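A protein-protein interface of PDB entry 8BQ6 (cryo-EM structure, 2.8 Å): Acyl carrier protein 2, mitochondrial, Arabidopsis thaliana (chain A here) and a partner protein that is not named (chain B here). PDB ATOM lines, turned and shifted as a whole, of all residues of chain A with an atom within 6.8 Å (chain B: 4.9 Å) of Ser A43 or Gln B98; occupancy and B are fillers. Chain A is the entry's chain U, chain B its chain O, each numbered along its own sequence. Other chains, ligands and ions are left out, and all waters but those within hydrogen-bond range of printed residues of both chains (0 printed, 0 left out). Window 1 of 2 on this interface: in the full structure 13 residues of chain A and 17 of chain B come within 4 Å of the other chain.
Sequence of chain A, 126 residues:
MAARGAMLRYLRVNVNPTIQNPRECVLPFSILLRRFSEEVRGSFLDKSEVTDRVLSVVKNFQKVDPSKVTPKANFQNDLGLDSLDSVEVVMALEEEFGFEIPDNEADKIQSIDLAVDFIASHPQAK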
ATOM      1  N   ARG A  41     -16.524   0.034  -9.825  1.00  0.00           N
ATOM      2  CA  ARG A  41     -17.695  -0.410  -9.020  1.00  0.00           C
ATOM      3  C   ARG A  41     -17.226  -0.959  -7.668  1.00  0.00           C
ATOM      4  O   ARG A  41     -16.015  -1.206  -7.518  1.00  0.00           O
ATOM      5  CB  ARG A  41     -18.502  -1.454  -9.796  1.00  0.00           C
ATOM      6  CG  ARG A  41     -19.149  -0.921 -11.067  1.00  0.00           C
ATOM      7  CD  ARG A  41     -19.864  -1.991 -11.872  1.00  0.00           C
ATOM      8  NE  ARG A  41     -20.994  -2.571 -11.161  1.00  0.00           N
ATOM      9  CZ  ARG A  41     -21.718  -3.599 -11.587  1.00  0.00           C
ATOM     10  NH1 ARG A  41     -21.438  -4.181 -12.741  1.00  0.00           N
ATOM     11  NH2 ARG A  41     -22.726  -4.040 -10.856  1.00  0.00           N
ATOM     12  N   GLY A  42     -18.155  -1.132  -6.721  1.00  0.00           N
ATOM     13  CA  GLY A  42     -17.824  -1.686  -5.393  1.00  0.00           C
ATOM     14  C   GLY A  42     -18.976  -2.508  -4.839  1.00  0.00           C
ATOM     15  O   GLY A  42     -20.116  -2.314  -5.309  1.00  0.00           O
ATOM     16  N   SER A  43     -18.703  -3.457  -3.957  1.00  0.00           N
ATOM     17  CA  SER A  43     -19.795  -4.339  -3.482  1.00  0.00           C
ATOM     18  C   SER A  43     -19.927  -4.187  -1.976  1.00  0.00           C
ATOM     19  O   SER A  43     -20.970  -4.568  -1.434  1.00  0.00           O
ATOM     20  CB  SER A  43     -19.522  -5.767  -3.855  1.00  0.00           C
ATOM     21  OG  SER A  43     -19.529  -5.944  -5.265  1.00  0.00           O
ATOM     22  N   PHE A  44     -18.909  -3.624  -1.333  1.00  0.00           N
ATOM     23  CA  PHE A  44     -18.918  -3.579   0.144  1.00  0.00           C
ATOM     24  C   PHE A  44     -18.862  -2.134   0.626  1.00  0.00           C
ATOM     25  O   PHE A  44     -18.243  -1.290  -0.048  1.00  0.00           O
ATOM     26  CB  PHE A  44     -17.764  -4.434   0.668  1.00  0.00           C
ATOM     27  CG  PHE A  44     -17.717  -5.819   0.077  1.00  0.00           C
ATOM     28  CD1 PHE A  44     -18.508  -6.831   0.589  1.00  0.00           C
ATOM     29  CD2 PHE A  44     -16.910  -6.099  -1.011  1.00  0.00           C
ATOM     30  CE1 PHE A  44     -18.483  -8.099   0.032  1.00  0.00           C
ATOM     31  CE2 PHE A  44     -16.896  -7.362  -1.571  1.00  0.00           C
ATOM     32  CZ  PHE A  44     -17.675  -8.362  -1.044  1.00  0.00           C
ATOM     33  N   LEU A  45     -19.530  -1.859   1.749  1.00  0.00           N
ATOM     34  CA  LEU A  45     -19.442  -0.514   2.364  1.00  0.00           C
ATOM     35  C   LEU A  45     -18.154  -0.496   3.180  1.00  0.00           C
ATOM     36  O   LEU A  45     -17.975  -1.436   3.984  1.00  0.00           O
ATOM     37  CB  LEU A  45     -20.655  -0.329   3.276  1.00  0.00           C
ATOM     38  CG  LEU A  45     -22.032  -0.296   2.620  1.00  0.00           C
ATOM     39  CD1 LEU A  45     -23.154  -0.255   3.645  1.00  0.00           C
ATOM     40  CD2 LEU A  45     -22.130   0.887   1.672  1.00  0.00           C
ATOM     41  N   ALA A 120     -19.766  -5.125   7.079  1.00  0.00           N
ATOM     42  CA  ALA A 120     -18.634  -4.687   6.230  1.00  0.00           C
ATOM     43  C   ALA A 120     -18.271  -5.740   5.181  1.00  0.00           C
ATOM     44  O   ALA A 120     -17.619  -5.371   4.186  1.00  0.00           O
ATOM     45  CB  ALA A 120     -17.448  -4.422   7.105  1.00  0.00           C
ATOM     46  N   SER A 121     -18.629  -7.000   5.416  1.00  0.00           N
ATOM     47  CA  SER A 121     -18.266  -8.105   4.493  1.00  0.00           C
ATOM     48  C   SER A 121     -19.509  -8.602   3.744  1.00  0.00           C
ATOM     49  O   SER A 121     -19.341  -9.385   2.803  1.00  0.00           O
ATOM     50  CB  SER A 121     -17.627  -9.203   5.276  1.00  0.00           C
ATOM     51  OG  SER A 121     -18.568  -9.790   6.164  1.00  0.00           O
ATOM     52  N   HIS A 122     -20.700  -8.179   4.172  1.00  0.00           N
ATOM     53  CA  HIS A 122     -21.961  -8.572   3.493  1.00  0.00           C
ATOM     54  C   HIS A 122     -22.188  -7.703   2.261  1.00  0.00           C
ATOM     55  O   HIS A 122     -22.220  -6.474   2.402  1.00  0.00           O
ATOM     56  CB  HIS A 122     -23.163  -8.434   4.416  1.00  0.00           C
ATOM     57  CG  HIS A 122     -24.132  -9.541   4.211  1.00  0.00           C
ATOM     58  ND1 HIS A 122     -25.040  -9.541   3.176  1.00  0.00           N
ATOM     59  CD2 HIS A 122     -24.307 -10.699   4.878  1.00  0.00           C
ATOM     60  CE1 HIS A 122     -25.751 -10.644   3.229  1.00  0.00           C
ATOM     61  NE2 HIS A 122     -25.323 -11.369   4.264  1.00  0.00           N
ATOM     62  N   PRO A 123     -22.276  -8.253   1.010  1.00  0.00           N
ATOM     63  CA  PRO A 123     -22.354  -7.409  -0.199  1.00  0.00           C
ATOM     64  C   PRO A 123     -23.703  -6.727  -0.470  1.00  0.00           C
ATOM     65  O   PRO A 123     -23.711  -5.752  -1.181  1.00  0.00           O
ATOM     66  CB  PRO A 123     -22.061  -8.382  -1.347  1.00  0.00           C
ATOM     67  CG  PRO A 123     -22.624  -9.686  -0.879  1.00  0.00           C
ATOM     68  CD  PRO A 123     -22.311  -9.689   0.598  1.00  0.00           C
ATOM     69  N   GLN A 124     -24.790  -7.252   0.094  1.00  0.00           N
ATOM     70  CA  GLN A 124     -26.142  -6.673  -0.086  1.00  0.00           C
ATOM     71  C   GLN A 124     -26.284  -5.413   0.769  1.00  0.00           C
ATOM     72  O   GLN A 124     -27.240  -4.655   0.529  1.00  0.00           O
ATOM     73  CB  GLN A 124     -27.178  -7.719   0.313  1.00  0.00           C
ATOM     74  CG  GLN A 124     -27.062  -9.008  -0.483  1.00  0.00           C
ATOM     75  CD  GLN A 124     -28.124 -10.011  -0.107  1.00  0.00           C
ATOM     76  OE1 GLN A 124     -28.536 -10.106   1.046  1.00  0.00           O
ATOM     77  NE2 GLN A 124     -28.568 -10.777  -1.087  1.00  0.00           N
ATOM     78  N   ALA A 125     -25.361  -5.202   1.707  1.00  0.00           N
ATOM     79  CA  ALA A 125     -25.383  -3.996   2.560  1.00  0.00           C
ATOM     80  C   ALA A 125     -25.076  -2.774   1.696  1.00  0.00           C
ATOM     81  O   ALA A 125     -23.943  -2.692   1.179  1.00  0.00           O
ATOM     82  CB  ALA A 125     -24.405  -4.146   3.694  1.00  0.00           C
ATOM     83  N   LYS A 126     -26.065  -1.895   1.528  1.00  0.00           N
ATOM     84  CA  LYS A 126     -25.922  -0.672   0.705  1.00  0.00           C
ATOM     85  C   LYS A 126     -27.090   0.272   1.025  1.00  0.00           C
ATOM     86  O   LYS A 126     -27.677   0.124   2.115  1.00  0.00           O
ATOM     87  CB  LYS A 126     -25.919  -1.004  -0.788  1.00  0.00           C
ATOM     88  CG  LYS A 126     -27.206  -1.608  -1.335  1.00  0.00           C
ATOM     89  CD  LYS A 126     -27.130  -1.884  -2.820  1.00  0.00           C
ATOM     90  CE  LYS A 126     -28.402  -2.485  -3.376  1.00  0.00           C
ATOM     91  NZ  LYS A 126     -28.293  -2.742  -4.830  1.00  0.00           N
ATOM     92  N   GLU B  96     -15.300 -15.561 -10.933  1.00  0.00           N
ATOM     93  CA  GLU B  96     -15.178 -14.254 -10.310  1.00  0.00           C
ATOM     94  C   GLU B  96     -15.859 -14.233  -8.948  1.00  0.00           C
ATOM     95  O   GLU B  96     -16.944 -14.788  -8.762  1.00  0.00           O
ATOM     96  CB  GLU B  96     -15.768 -13.190 -11.233  1.00  0.00           C
ATOM     97  CG  GLU B  96     -16.118 -11.886 -10.565  1.00  0.00           C
ATOM     98  CD  GLU B  96     -16.755 -10.907 -11.529  1.00  0.00           C
ATOM     99  OE1 GLU B  96     -17.190 -11.333 -12.618  1.00  0.00           O
ATOM    100  OE2 GLU B  96     -16.815  -9.706 -11.201  1.00  0.00           O
ATOM    101  N   VAL B  97     -15.187 -13.607  -7.980  1.00  0.00           N
ATOM    102  CA  VAL B  97     -15.703 -13.444  -6.630  1.00  0.00           C
ATOM    103  C   VAL B  97     -15.442 -12.010  -6.197  1.00  0.00           C
ATOM    104  O   VAL B  97     -14.577 -11.321  -6.740  1.00  0.00           O
ATOM    105  CB  VAL B  97     -15.050 -14.422  -5.630  1.00  0.00           C
ATOM    106  CG1 VAL B  97     -15.431 -15.854  -5.951  1.00  0.00           C
ATOM    107  CG2 VAL B  97     -13.544 -14.247  -5.629  1.00  0.00           C
ATOM    108  N   GLN B  98     -16.194 -11.564  -5.195  1.00  0.00           N
ATOM    109  CA  GLN B  98     -16.009 -10.243  -4.611  1.00  0.00           C
ATOM    110  C   GLN B  98     -15.493 -10.377  -3.187  1.00  0.00           C
ATOM    111  O   GLN B  98     -16.017 -11.174  -2.401  1.00  0.00           O
ATOM    112  CB  GLN B  98     -17.302  -9.437  -4.623  1.00  0.00           C
ATOM    113  CG  GLN B  98     -17.550  -8.747  -5.931  1.00  0.00           C
ATOM    114  CD  GLN B  98     -18.373  -9.609  -6.845  1.00  0.00           C
ATOM    115  OE1 GLN B  98     -19.370 -10.192  -6.424  1.00  0.00           O
ATOM    116  NE2 GLN B  98     -17.956  -9.716  -8.098  1.00  0.00           N
ATOM    117  N   ILE B  99     -14.473  -9.588  -2.859  1.00  0.00           N
ATOM    118  CA  ILE B  99     -13.777  -9.664  -1.581  1.00  0.00           C
ATOM    119  C   ILE B  99     -13.606  -8.257  -1.027  1.00  0.00           C
ATOM    120  O   ILE B  99     -13.313  -7.320  -1.778  1.00  0.00           O
ATOM    121  CB  ILE B  99     -12.411 -10.358  -1.724  1.00  0.00           C
ATOM    122  CG1 ILE B  99     -12.576 -11.715  -2.408  1.00  0.00           C
ATOM    123  CG2 ILE B  99     -11.759 -10.527  -0.375  1.00  0.00           C
ATOM    124  CD1 ILE B  99     -11.293 -12.430  -2.654  1.00  0.00           C
ATOM    125  N   ALA B 100     -13.778  -8.112   0.285  1.00  0.00           N
ATOM    126  CA  ALA B 100     -13.630  -6.820   0.936  1.00  0.00           C
ATOM    127  C   ALA B 100     -12.166  -6.387   0.979  1.00  0.00           C
ATOM    128  O   ALA B 100     -11.242  -7.205   0.943  1.00  0.00           O
ATOM    129  CB  ALA B 100     -14.201  -6.866   2.351  1.00  0.00           C
ATOM    130  N   ASN B 128     -14.882  -3.870 -11.530  1.00  0.00           N
ATOM    131  CA  ASN B 128     -15.217  -3.766 -10.119  1.00  0.00           C
ATOM    132  C   ASN B 128     -13.944  -3.858  -9.287  1.00  0.00           C
ATOM    133  O   ASN B 128     -13.140  -4.776  -9.471  1.00  0.00           O
ATOM    134  CB  ASN B 128     -16.187  -4.882  -9.743  1.00  0.00           C
ATOM    135  CG  ASN B 128     -16.828  -4.673  -8.398  1.00  0.00           C
ATOM    136  OD1 ASN B 128     -16.185  -4.239  -7.445  1.00  0.00           O
ATOM    137  ND2 ASN B 128     -18.105  -5.004  -8.304  1.00  0.00           N
ATOM    138  N   HIS B 130     -13.576  -4.627  -6.186  1.00  0.00           N
ATOM    139  CA  HIS B 130     -13.571  -5.745  -5.252  1.00  0.00           C
ATOM    140  C   HIS B 130     -13.675  -7.091  -5.943  1.00  0.00           C
ATOM    141  O   HIS B 130     -13.880  -8.104  -5.271  1.00  0.00           O
ATOM    142  CB  HIS B 130     -14.703  -5.602  -4.243  1.00  0.00           C
ATOM    143  CG  HIS B 130     -14.575  -4.392  -3.378  1.00  0.00           C
ATOM    144  ND1 HIS B 130     -15.436  -3.320  -3.465  1.00  0.00           N
ATOM    145  CD2 HIS B 130     -13.661  -4.067  -2.437  1.00  0.00           C
ATOM    146  CE1 HIS B 130     -15.072  -2.397  -2.595  1.00  0.00           C
ATOM    147  NE2 HIS B 130     -13.995  -2.824  -1.960  1.00  0.00           N
ATOM    148  N   SER B 131     -13.545  -7.125  -7.262  1.00  0.00           N
ATOM    149  CA  SER B 131     -13.635  -8.364  -8.013  1.00  0.00           C
ATOM    150  C   SER B 131     -12.260  -8.989  -8.177  1.00  0.00           C
ATOM    151  O   SER B 131     -11.283  -8.302  -8.487  1.00  0.00           O
ATOM    152  CB  SER B 131     -14.254  -8.115  -9.387  1.00  0.00           C
ATOM    153  OG  SER B 131     -15.664  -8.215  -9.335  1.00  0.00           O
ATOM    154  N   VAL B 147     -13.369 -13.792   3.929  1.00  0.00           N
ATOM    155  CA  VAL B 147     -14.773 -13.866   3.541  1.00  0.00           C
ATOM    156  C   VAL B 147     -14.889 -13.474   2.079  1.00  0.00           C
ATOM    157  O   VAL B 147     -14.281 -12.490   1.640  1.00  0.00           O
ATOM    158  CB  VAL B 147     -15.658 -12.974   4.424  1.00  0.00           C
ATOM    159  CG1 VAL B 147     -17.107 -13.056   3.967  1.00  0.00           C
ATOM    160  CG2 VAL B 147     -15.549 -13.403   5.866  1.00  0.00           C
ATOM    161  N   VAL B 148     -15.667 -14.243   1.328  1.00  0.00           N
ATOM    162  CA  VAL B 148     -15.767 -14.103  -0.115  1.00  0.00           C
ATOM    163  C   VAL B 148     -17.242 -14.047  -0.487  1.00  0.00           C
ATOM    164  O   VAL B 148     -18.074 -14.712   0.139  1.00  0.00           O
ATOM    165  CB  VAL B 148     -15.045 -15.271  -0.820  1.00  0.00           C
ATOM    166  CG1 VAL B 148     -15.553 -15.467  -2.226  1.00  0.00           C
ATOM    167  CG2 VAL B 148     -13.545 -15.044  -0.803  1.00  0.00           C
ATOM    168  N   ALA B 149     -17.572 -13.219  -1.471  1.00  0.00           N
ATOM    169  CA  ALA B 149     -18.924 -13.137  -2.002  1.00  0.00           C
ATOM    170  C   ALA B 149     -18.955 -13.741  -3.399  1.00  0.00           C
ATOM    171  O   ALA B 149     -18.130 -13.393  -4.250  1.00  0.00           O
ATOM    172  CB  ALA B 149     -19.410 -11.689  -2.037  1.00  0.00           C
ATOM    173  N   PRO B 151     -21.024 -14.059  -6.766  1.00  0.00           N
ATOM    174  CA  PRO B 151     -22.150 -13.472  -7.496  1.00  0.00           C
ATOM    175  C   PRO B 151     -22.931 -14.534  -8.262  1.00  0.00           C
ATOM    176  O   PRO B 151     -22.600 -15.720  -8.256  1.00  0.00           O
ATOM    177  CB  PRO B 151     -21.477 -12.480  -8.447  1.00  0.00           C
ATOM    178  CG  PRO B 151     -20.112 -13.026  -8.653  1.00  0.00           C
ATOM    179  CD  PRO B 151     -19.729 -13.759  -7.400  1.00  0.00           C
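Printed residues of chain B that touch a printed residue of chain A: Gln B98, Ile B99, Ala B100, Asn B128, His B130 and Ala B149. Hydrophobic or aromatic side chains of chain B that line the printed part of chain A: His B130 and Ala B149. Hydrophobic or aromatic side chains of chain A within 4 Å of the printed part of chain B: Phe A44 and Pro A123. Along chain A the printed residues that touch a printed residue of chain B span positions 41 to 123. Among the printed residues, no Asp or Glu carboxylate lies within 4 Å of a Lys or Arg side-chain nitrogen of the other chain.
The side-chain carboxylate (OE2) of Glu B96 lies within hydrogen-bond range of the side-chain amide nitrogen (NE2) of Gln B98 (3.3 Å). The backbone carbonyl oxygen (O) of His B130 lies within hydrogen-bond range of the backbone NH (N) of Ile B99 (2.9 Å). The backbone carbonyl oxygen of Gln B98 is in hydrogen-bond range of the backbone NH of Ala B149. NE2 of Gln B98 sits at hydrogen-bond distance from OG of Ser B131. OD1 of Asn B128 is in hydrogen-bond range of N of His B130, 2.9 Å away.
ND2 of Asn B128 sits at hydrogen-bond distance from OG of Ser A43, at 3.5 Å. The backbone NH of Ser A43 is in hydrogen-bond range of a ring nitrogen (ND1) of His B130 (3.3 Å). O of Arg A41 lies close to OD1 of Asn B128, at 3.0 Å.
Of chain A, only Ser A43 and Phe A44 come within 4 Å of Gln B98. Of the printed residues of chain A, Ala B100 touches Phe A44. Printed residues of chain A within 4 Å of Ile B99: Phe A44. Printed residues of chain A within 4 Å of Ala B149: Phe A44 and Pro A123. The nearest residue of chain A that does not touch Gln B98 is Pro A123 (5.9 Å).
Among the printed residues, pairs that only touch across the chains: Phe A44 with Ile B99 (3.5 Å), Gly A42 with His B130 (3.5 Å), Ser A43 with Gln B98 (3.5 Å), Phe A44 with Gln B98 (3.5 Å), Gly A42 with Asn B128 (3.7 Å), Phe A44 with Ala B100 (3.7 Å), Phe A44 with His B130 (3.7 Å), Phe A44 with Ala B149 (3.9 Å) and Pro A123 with Ala B149 (3.96 Å).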
